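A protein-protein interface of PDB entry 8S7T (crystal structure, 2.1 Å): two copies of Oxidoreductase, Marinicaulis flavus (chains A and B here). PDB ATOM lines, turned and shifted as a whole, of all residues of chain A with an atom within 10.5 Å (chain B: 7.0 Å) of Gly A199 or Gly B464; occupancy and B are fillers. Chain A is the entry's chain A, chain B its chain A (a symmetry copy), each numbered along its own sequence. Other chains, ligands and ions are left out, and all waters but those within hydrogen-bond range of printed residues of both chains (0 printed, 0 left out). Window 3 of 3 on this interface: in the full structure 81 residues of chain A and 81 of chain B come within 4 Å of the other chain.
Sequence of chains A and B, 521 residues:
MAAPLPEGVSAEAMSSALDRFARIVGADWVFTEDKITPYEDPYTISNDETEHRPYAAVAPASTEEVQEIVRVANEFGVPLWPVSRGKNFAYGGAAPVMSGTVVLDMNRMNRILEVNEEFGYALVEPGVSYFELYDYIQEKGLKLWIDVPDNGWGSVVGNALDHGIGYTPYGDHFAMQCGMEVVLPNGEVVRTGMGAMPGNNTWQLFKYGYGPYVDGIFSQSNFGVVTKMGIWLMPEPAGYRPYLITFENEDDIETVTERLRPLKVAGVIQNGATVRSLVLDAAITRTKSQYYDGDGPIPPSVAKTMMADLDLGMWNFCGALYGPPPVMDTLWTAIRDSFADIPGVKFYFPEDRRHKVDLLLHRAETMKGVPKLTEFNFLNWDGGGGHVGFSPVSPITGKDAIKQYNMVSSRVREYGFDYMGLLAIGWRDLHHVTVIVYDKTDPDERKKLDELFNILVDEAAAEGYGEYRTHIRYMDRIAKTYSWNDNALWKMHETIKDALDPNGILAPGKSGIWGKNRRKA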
ATOM      1  N   ARG A 191     -10.831  21.107  -3.152  1.00  0.00           N
ATOM      2  CA  ARG A 191     -10.628  20.872  -4.563  1.00  0.00           C
ATOM      3  C   ARG A 191     -11.046  19.452  -4.895  1.00  0.00           C
ATOM      4  O   ARG A 191     -10.733  18.511  -4.173  1.00  0.00           O
ATOM      5  CB  ARG A 191      -9.184  21.144  -4.944  1.00  0.00           C
ATOM      6  CG  ARG A 191      -8.818  22.609  -4.835  1.00  0.00           C
ATOM      7  CD  ARG A 191      -7.374  22.859  -5.205  1.00  0.00           C
ATOM      8  NE  ARG A 191      -7.094  24.281  -5.240  1.00  0.00           N
ATOM      9  CZ  ARG A 191      -5.985  24.825  -5.707  1.00  0.00           C
ATOM     10  NH1 ARG A 191      -5.025  24.067  -6.206  1.00  0.00           N
ATOM     11  NH2 ARG A 191      -5.869  26.142  -5.709  1.00  0.00           N
ATOM     12  N   GLY A 193     -11.553  16.029  -7.499  1.00  0.00           N
ATOM     13  CA  GLY A 193     -10.815  15.238  -8.465  1.00  0.00           C
ATOM     14  C   GLY A 193      -9.336  15.171  -8.091  1.00  0.00           C
ATOM     15  O   GLY A 193      -8.960  15.031  -6.924  1.00  0.00           O
ATOM     16  N   MET A 194      -8.504  15.267  -9.119  1.00  0.00           N
ATOM     17  CA  MET A 194      -7.068  15.205  -8.968  1.00  0.00           C
ATOM     18  C   MET A 194      -6.539  16.473  -8.291  1.00  0.00           C
ATOM     19  O   MET A 194      -5.425  16.476  -7.784  1.00  0.00           O
ATOM     20  CB  MET A 194      -6.416  15.064 -10.343  1.00  0.00           C
ATOM     21  CG  MET A 194      -6.880  13.829 -11.098  1.00  0.00           C
ATOM     22  SD  MET A 194      -6.799  12.288 -10.177  1.00  0.00           S
ATOM     23  CE  MET A 194      -5.074  12.167  -9.723  1.00  0.00           C
ATOM     24  N   GLY A 195      -7.327  17.552  -8.244  1.00  0.00           N
ATOM     25  CA  GLY A 195      -6.843  18.755  -7.593  1.00  0.00           C
ATOM     26  C   GLY A 195      -6.737  18.585  -6.080  1.00  0.00           C
ATOM     27  O   GLY A 195      -6.051  19.353  -5.416  1.00  0.00           O
ATOM     28  N   ALA A 196      -7.382  17.552  -5.542  1.00  0.00           N
ATOM     29  CA  ALA A 196      -7.243  17.222  -4.128  1.00  0.00           C
ATOM     30  C   ALA A 196      -5.886  16.583  -3.848  1.00  0.00           C
ATOM     31  O   ALA A 196      -5.482  16.418  -2.686  1.00  0.00           O
ATOM     32  CB  ALA A 196      -8.348  16.303  -3.699  1.00  0.00           C
ATOM     33  N   MET A 197      -5.176  16.204  -4.916  1.00  0.00           N
ATOM     34  CA  MET A 197      -3.864  15.617  -4.724  1.00  0.00           C
ATOM     35  C   MET A 197      -2.819  16.699  -4.967  1.00  0.00           C
ATOM     36  O   MET A 197      -2.703  17.182  -6.087  1.00  0.00           O
ATOM     37  CB  MET A 197      -3.611  14.445  -5.678  1.00  0.00           C
ATOM     38  CG  MET A 197      -2.196  13.974  -5.609  1.00  0.00           C
ATOM     39  SD  MET A 197      -1.821  12.754  -6.863  1.00  0.00           S
ATOM     40  CE  MET A 197      -0.166  12.366  -6.317  1.00  0.00           C
ATOM     41  N   PRO A 198      -2.005  17.084  -3.952  1.00  0.00           N
ATOM     42  CA  PRO A 198      -1.005  18.140  -4.129  1.00  0.00           C
ATOM     43  C   PRO A 198       0.059  17.679  -5.125  1.00  0.00           C
ATOM     44  O   PRO A 198       0.430  16.518  -5.142  1.00  0.00           O
ATOM     45  CB  PRO A 198      -0.419  18.333  -2.720  1.00  0.00           C
ATOM     46  CG  PRO A 198      -1.366  17.611  -1.788  1.00  0.00           C
ATOM     47  CD  PRO A 198      -1.943  16.483  -2.613  1.00  0.00           C
ATOM     48  N   GLY A 199       0.525  18.571  -5.991  1.00  0.00           N
ATOM     49  CA  GLY A 199       1.573  18.231  -6.944  1.00  0.00           C
ATOM     50  C   GLY A 199       1.074  17.568  -8.234  1.00  0.00           C
ATOM     51  O   GLY A 199       1.892  17.166  -9.056  1.00  0.00           O
ATOM     52  N   ASN A 200      -0.249  17.448  -8.433  1.00  0.00           N
ATOM     53  CA  ASN A 200      -0.792  16.842  -9.649  1.00  0.00           C
ATOM     54  C   ASN A 200      -0.651  17.835 -10.804  1.00  0.00           C
ATOM     55  O   ASN A 200      -0.657  19.041 -10.596  1.00  0.00           O
ATOM     56  CB  ASN A 200      -2.276  16.469  -9.505  1.00  0.00           C
ATOM     57  CG  ASN A 200      -3.166  17.684  -9.690  1.00  0.00           C
ATOM     58  OD1 ASN A 200      -3.472  18.079 -10.808  1.00  0.00           O
ATOM     59  ND2 ASN A 200      -3.540  18.344  -8.607  1.00  0.00           N
ATOM     60  N   ASN A 201      -0.549  17.309 -12.024  1.00  0.00           N
ATOM     61  CA  ASN A 201      -0.700  18.067 -13.240  1.00  0.00           C
ATOM     62  C   ASN A 201      -1.904  17.525 -14.000  1.00  0.00           C
ATOM     63  O   ASN A 201      -1.910  17.553 -15.219  1.00  0.00           O
ATOM     64  CB  ASN A 201       0.571  17.983 -14.093  1.00  0.00           C
ATOM     65  CG  ASN A 201       1.749  18.680 -13.439  1.00  0.00           C
ATOM     66  OD1 ASN A 201       2.704  18.040 -13.013  1.00  0.00           O
ATOM     67  ND2 ASN A 201       1.671  19.989 -13.298  1.00  0.00           N
ATOM     68  N   THR A 202      -2.892  16.985 -13.284  1.00  0.00           N
ATOM     69  CA  THR A 202      -3.934  16.190 -13.908  1.00  0.00           C
ATOM     70  C   THR A 202      -5.334  16.716 -13.573  1.00  0.00           C
ATOM     71  O   THR A 202      -6.334  16.102 -13.948  1.00  0.00           O
ATOM     72  CB  THR A 202      -3.767  14.711 -13.508  1.00  0.00           C
ATOM     73  OG1 THR A 202      -3.655  14.623 -12.090  1.00  0.00           O
ATOM     74  CG2 THR A 202      -2.552  14.077 -14.138  1.00  0.00           C
ATOM     75  N   TRP A 203      -5.417  17.870 -12.907  1.00  0.00           N
ATOM     76  CA  TRP A 203      -6.683  18.421 -12.446  1.00  0.00           C
ATOM     77  C   TRP A 203      -7.683  18.573 -13.589  1.00  0.00           C
ATOM     78  O   TRP A 203      -8.864  18.285 -13.406  1.00  0.00           O
ATOM     79  CB  TRP A 203      -6.455  19.764 -11.743  1.00  0.00           C
ATOM     80  CG  TRP A 203      -7.538  20.186 -10.796  1.00  0.00           C
ATOM     81  CD1 TRP A 203      -8.603  19.470 -10.326  1.00  0.00           C
ATOM     82  CD2 TRP A 203      -7.645  21.490 -10.204  1.00  0.00           C
ATOM     83  NE1 TRP A 203      -9.333  20.220  -9.436  1.00  0.00           N
ATOM     84  CE2 TRP A 203      -8.773  21.471  -9.353  1.00  0.00           C
ATOM     85  CE3 TRP A 203      -6.868  22.650 -10.283  1.00  0.00           C
ATOM     86  CZ2 TRP A 203      -9.146  22.591  -8.609  1.00  0.00           C
ATOM     87  CZ3 TRP A 203      -7.237  23.752  -9.541  1.00  0.00           C
ATOM     88  CH2 TRP A 203      -8.366  23.721  -8.724  1.00  0.00           C
ATOM     89  N   LEU A 205      -7.496  16.798 -16.470  1.00  0.00           N
ATOM     90  CA  LEU A 205      -7.305  15.683 -17.397  1.00  0.00           C
ATOM     91  C   LEU A 205      -8.167  14.482 -17.031  1.00  0.00           C
ATOM     92  O   LEU A 205      -8.391  13.591 -17.857  1.00  0.00           O
ATOM     93  CB  LEU A 205      -5.831  15.275 -17.419  1.00  0.00           C
ATOM     94  CG  LEU A 205      -4.843  16.357 -17.834  1.00  0.00           C
ATOM     95  CD1 LEU A 205      -3.462  15.758 -17.933  1.00  0.00           C
ATOM     96  CD2 LEU A 205      -5.226  17.020 -19.142  1.00  0.00           C
ATOM     97  N   PHE A 206      -8.624  14.425 -15.782  1.00  0.00           N
ATOM     98  CA  PHE A 206      -9.335  13.251 -15.315  1.00  0.00           C
ATOM     99  C   PHE A 206     -10.352  13.710 -14.279  1.00  0.00           C
ATOM    100  O   PHE A 206      -9.963  14.258 -13.248  1.00  0.00           O
ATOM    101  CB  PHE A 206      -8.320  12.226 -14.781  1.00  0.00           C
ATOM    102  CG  PHE A 206      -8.909  10.927 -14.279  1.00  0.00           C
ATOM    103  CD1 PHE A 206      -9.332   9.950 -15.163  1.00  0.00           C
ATOM    104  CD2 PHE A 206      -9.073  10.696 -12.923  1.00  0.00           C
ATOM    105  CE1 PHE A 206      -9.885   8.765 -14.700  1.00  0.00           C
ATOM    106  CE2 PHE A 206      -9.636   9.513 -12.466  1.00  0.00           C
ATOM    107  CZ  PHE A 206     -10.027   8.544 -13.350  1.00  0.00           C
ATOM    108  N   PRO B 392      -2.392   4.711 -11.514  1.00  0.00           N
ATOM    109  CA  PRO B 392      -2.474   6.163 -11.294  1.00  0.00           C
ATOM    110  C   PRO B 392      -2.625   6.987 -12.572  1.00  0.00           C
ATOM    111  O   PRO B 392      -2.237   6.561 -13.663  1.00  0.00           O
ATOM    112  CB  PRO B 392      -1.118   6.494 -10.646  1.00  0.00           C
ATOM    113  CG  PRO B 392      -0.205   5.444 -11.224  1.00  0.00           C
ATOM    114  CD  PRO B 392      -1.059   4.182 -11.203  1.00  0.00           C
ATOM    115  N   VAL B 393      -3.142   8.203 -12.392  1.00  0.00           N
ATOM    116  CA  VAL B 393      -3.352   9.122 -13.490  1.00  0.00           C
ATOM    117  C   VAL B 393      -2.097   9.968 -13.692  1.00  0.00           C
ATOM    118  O   VAL B 393      -1.458  10.367 -12.729  1.00  0.00           O
ATOM    119  CB  VAL B 393      -4.574  10.006 -13.182  1.00  0.00           C
ATOM    120  CG1 VAL B 393      -4.915  10.910 -14.337  1.00  0.00           C
ATOM    121  CG2 VAL B 393      -5.780   9.171 -12.799  1.00  0.00           C
ATOM    122  N   SER B 394      -1.798  10.299 -14.947  1.00  0.00           N
ATOM    123  CA  SER B 394      -0.686  11.168 -15.289  1.00  0.00           C
ATOM    124  C   SER B 394      -1.022  11.916 -16.571  1.00  0.00           C
ATOM    125  O   SER B 394      -1.985  11.562 -17.236  1.00  0.00           O
ATOM    126  CB  SER B 394       0.570  10.373 -15.457  1.00  0.00           C
ATOM    127  OG  SER B 394       0.374   9.383 -16.441  1.00  0.00           O
ATOM    128  N   PRO B 395      -0.318  13.021 -16.902  1.00  0.00           N
ATOM    129  CA  PRO B 395      -0.469  13.663 -18.212  1.00  0.00           C
ATOM    130  C   PRO B 395      -0.058  12.759 -19.375  1.00  0.00           C
ATOM    131  O   PRO B 395       0.874  11.968 -19.250  1.00  0.00           O
ATOM    132  CB  PRO B 395       0.467  14.899 -18.138  1.00  0.00           C
ATOM    133  CG  PRO B 395       0.624  15.159 -16.640  1.00  0.00           C
ATOM    134  CD  PRO B 395       0.542  13.792 -15.978  1.00  0.00           C
ATOM    135  N   LYS B 403       9.182   7.840 -17.550  1.00  0.00           N
ATOM    136  CA  LYS B 403       9.541   7.914 -16.144  1.00  0.00           C
ATOM    137  C   LYS B 403       8.833   6.830 -15.326  1.00  0.00           C
ATOM    138  O   LYS B 403       9.443   6.186 -14.475  1.00  0.00           O
ATOM    139  CB  LYS B 403       9.200   9.281 -15.552  1.00  0.00           C
ATOM    140  CG  LYS B 403       9.719   9.455 -14.130  1.00  0.00           C
ATOM    141  CD  LYS B 403       8.884  10.369 -13.307  1.00  0.00           C
ATOM    142  CE  LYS B 403       8.972  11.814 -13.735  1.00  0.00           C
ATOM    143  NZ  LYS B 403       7.964  12.623 -13.006  1.00  0.00           N
ATOM    144  N   GLU B 459       6.055   6.346  -4.232  1.00  0.00           N
ATOM    145  CA  GLU B 459       6.939   6.958  -5.198  1.00  0.00           C
ATOM    146  C   GLU B 459       6.159   7.591  -6.341  1.00  0.00           C
ATOM    147  O   GLU B 459       6.556   8.630  -6.872  1.00  0.00           O
ATOM    148  CB  GLU B 459       7.967   5.933  -5.673  1.00  0.00           C
ATOM    149  CG  GLU B 459       8.902   5.576  -4.538  1.00  0.00           C
ATOM    150  CD  GLU B 459      10.087   4.682  -4.828  1.00  0.00           C
ATOM    151  OE1 GLU B 459      10.109   4.010  -5.894  1.00  0.00           O
ATOM    152  OE2 GLU B 459      10.987   4.659  -3.956  1.00  0.00           O
ATOM    153  N   ALA B 460       5.046   6.971  -6.722  1.00  0.00           N
ATOM    154  CA  ALA B 460       4.245   7.531  -7.788  1.00  0.00           C
ATOM    155  C   ALA B 460       3.601   8.834  -7.290  1.00  0.00           C
ATOM    156  O   ALA B 460       3.596   9.833  -8.016  1.00  0.00           O
ATOM    157  CB  ALA B 460       3.248   6.500  -8.267  1.00  0.00           C
ATOM    158  N   ALA B 461       3.120   8.835  -6.032  1.00  0.00           N
ATOM    159  CA  ALA B 461       2.399   9.981  -5.487  1.00  0.00           C
ATOM    160  C   ALA B 461       3.308  11.215  -5.477  1.00  0.00           C
ATOM    161  O   ALA B 461       2.874  12.304  -5.812  1.00  0.00           O
ATOM    162  CB  ALA B 461       1.839   9.673  -4.115  1.00  0.00           C
ATOM    163  N   ALA B 462       4.590  11.013  -5.181  1.00  0.00           N
ATOM    164  CA  ALA B 462       5.551  12.090  -5.033  1.00  0.00           C
ATOM    165  C   ALA B 462       5.905  12.692  -6.389  1.00  0.00           C
ATOM    166  O   ALA B 462       6.367  13.828  -6.474  1.00  0.00           O
ATOM    167  CB  ALA B 462       6.785  11.550  -4.331  1.00  0.00           C
ATOM    168  N   GLU B 463       5.702  11.924  -7.460  1.00  0.00           N
ATOM    169  CA  GLU B 463       5.886  12.445  -8.806  1.00  0.00           C
ATOM    170  C   GLU B 463       4.591  13.062  -9.336  1.00  0.00           C
ATOM    171  O   GLU B 463       4.556  13.496 -10.484  1.00  0.00           O
ATOM    172  CB  GLU B 463       6.379  11.317  -9.706  1.00  0.00           C
ATOM    173  CG  GLU B 463       7.727  10.768  -9.281  1.00  0.00           C
ATOM    174  CD  GLU B 463       8.850  11.788  -9.293  1.00  0.00           C
ATOM    175  OE1 GLU B 463       8.843  12.649 -10.185  1.00  0.00           O
ATOM    176  OE2 GLU B 463       9.742  11.704  -8.435  1.00  0.00           O
ATOM    177  N   GLY B 464       3.534  13.071  -8.511  1.00  0.00           N
ATOM    178  CA  GLY B 464       2.258  13.684  -8.875  1.00  0.00           C
ATOM    179  C   GLY B 464       1.253  12.736  -9.550  1.00  0.00           C
ATOM    180  O   GLY B 464       0.336  13.197 -10.219  1.00  0.00           O
ATOM    181  N   TYR B 465       1.389  11.420  -9.338  1.00  0.00           N
ATOM    182  CA  TYR B 465       0.527  10.450  -9.996  1.00  0.00           C
ATOM    183  C   TYR B 465      -0.325   9.751  -8.950  1.00  0.00           C
ATOM    184  O   TYR B 465       0.196   9.029  -8.100  1.00  0.00           O
ATOM    185  CB  TYR B 465       1.355   9.414 -10.763  1.00  0.00           C
ATOM    186  CG  TYR B 465       2.408   9.986 -11.674  1.00  0.00           C
ATOM    187  CD1 TYR B 465       2.181  11.148 -12.403  1.00  0.00           C
ATOM    188  CD2 TYR B 465       3.636   9.358 -11.826  1.00  0.00           C
ATOM    189  CE1 TYR B 465       3.152  11.691 -13.232  1.00  0.00           C
ATOM    190  CE2 TYR B 465       4.610   9.884 -12.666  1.00  0.00           C
ATOM    191  CZ  TYR B 465       4.372  11.052 -13.373  1.00  0.00           C
ATOM    192  OH  TYR B 465       5.338  11.555 -14.219  1.00  0.00           O
ATOM    193  N   GLY B 466      -1.640   9.967  -9.021  1.00  0.00           N
ATOM    194  CA  GLY B 466      -2.545   9.454  -8.012  1.00  0.00           C
ATOM    195  C   GLY B 466      -3.452   8.354  -8.548  1.00  0.00           C
ATOM    196  O   GLY B 466      -3.896   8.401  -9.701  1.00  0.00           O
ATOM    197  N   TRP B 484      -4.774  17.533  -0.121  1.00  0.00           N
ATOM    198  CA  TRP B 484      -4.658  18.985  -0.205  1.00  0.00           C
ATOM    199  C   TRP B 484      -5.509  19.669   0.868  1.00  0.00           C
ATOM    200  O   TRP B 484      -6.670  19.314   1.069  1.00  0.00           O
ATOM    201  CB  TRP B 484      -5.045  19.479  -1.592  1.00  0.00           C
ATOM    202  CG  TRP B 484      -4.815  20.943  -1.788  1.00  0.00           C
ATOM    203  CD1 TRP B 484      -3.650  21.557  -2.131  1.00  0.00           C
ATOM    204  CD2 TRP B 484      -5.804  21.979  -1.652  1.00  0.00           C
ATOM    205  NE1 TRP B 484      -3.851  22.910  -2.237  1.00  0.00           N
ATOM    206  CE2 TRP B 484      -5.161  23.198  -1.939  1.00  0.00           C
ATOM    207  CE3 TRP B 484      -7.169  21.990  -1.329  1.00  0.00           C
ATOM    208  CZ2 TRP B 484      -5.841  24.419  -1.914  1.00  0.00           C
ATOM    209  CZ3 TRP B 484      -7.832  23.198  -1.312  1.00  0.00           C
ATOM    210  CH2 TRP B 484      -7.178  24.397  -1.590  1.00  0.00           C
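The backbone carbonyl oxygen of Ala A196 is in hydrogen-bond range of the backbone NH of Trp B484, 2.9 Å away.
N of Gly B466 sits at hydrogen-bond distance from SD of Met A197 (3.5 Å).
No position is printed for both chains.
Of the 14 printed residues of chain A, 12 touch a printed residue of chain B.
Printed residues of chain B that touch a printed residue of chain A: Val B393, Ser B394, Pro B395, Ala B461, Gly B464, Tyr B465, Gly B466 and Trp B484.
Along chain B the printed residues that touch a printed residue of chain A span positions 393 to 484.
Gly A199 touches just one residue of chain B: Gly B464.
No residue of chain A comes within 4 Å of Ala B462.
Of the printed residues of chain B, Thr A202 touches Val B393, Ser B394 and Pro B395.
Of the printed residues of chain B, Pro A198 touches Trp B484.
Printed residues of chain B within 4 Å of Met A197: Ala B461 (3.1 Å), Gly B464 (3.6 Å), Tyr B465 (3.5 Å) and Gly B466 (3.5 Å).
Of the printed residues of chain B, Arg A191 touches Trp B484.
Trp A203 touches none of the printed residues of chain B.
Lys B403 touches none of the printed residues of chain A.
The nearest residue of chain B that does not touch Gly A199 is Glu B463 (4.8 Å).
The nearest residue of chain A that does not touch Gly B464 is Asn A201 (4.6 Å).
The nearest printed residue of chain B that does not touch Ala A196 is Gly B466 (8.9 Å).
Among the printed residues, pairs that only touch across the chains: Arg A191 with Trp B484 (3.6 Å), Met A194 with Gly B466 (3.9 Å), Gly A195 with Trp B484 (3.96 Å), Met A197 with Ala B461 (3.1 Å), Met A197 with Gly B464 (3.6 Å), Met A197 with Tyr B465 (3.5 Å), Pro A198 with Trp B484 (3.8 Å), Gly A199 with Gly B464 (3.5 Å), Asn A200 with Gly B464 (3.9 Å), Asn A201 with Pro B395 (3.8 Å), Thr A202 with Val B393 (3.96 Å), Thr A202 with Ser B394 (3.6 Å), Thr A202 with Pro B395 (3.6 Å), Leu A205 with Pro B395 (3.7 Å) and Phe A206 with Val B393 (3.6 Å).
The side-chain amide nitrogen of Asn A200 sits at hydrogen-bond distance from the backbone carbonyl oxygen of Met A194.
The backbone carbonyl oxygen (O) of Met A197 is in hydrogen-bond range of the side-chain amide nitrogen (ND2) of Asn A200 (2.9 Å).
The backbone NH of Thr A202 lies within hydrogen-bond range of the side-chain amide oxygen of Asn A200 (2.8 Å).
The backbone carbonyl oxygen (O) of Gly B466 is in hydrogen-bond range of the backbone NH (N) of Val B393, at 2.8 Å.
The side-chain amino group (NZ) of Lys B403 sits at hydrogen-bond distance from the side-chain hydroxyl (OH) of Tyr B465 (3.1 Å).
The backbone NH (N) of Tyr B465 is in hydrogen-bond range of the backbone carbonyl oxygen (O) of Ala B460 (3.0 Å).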
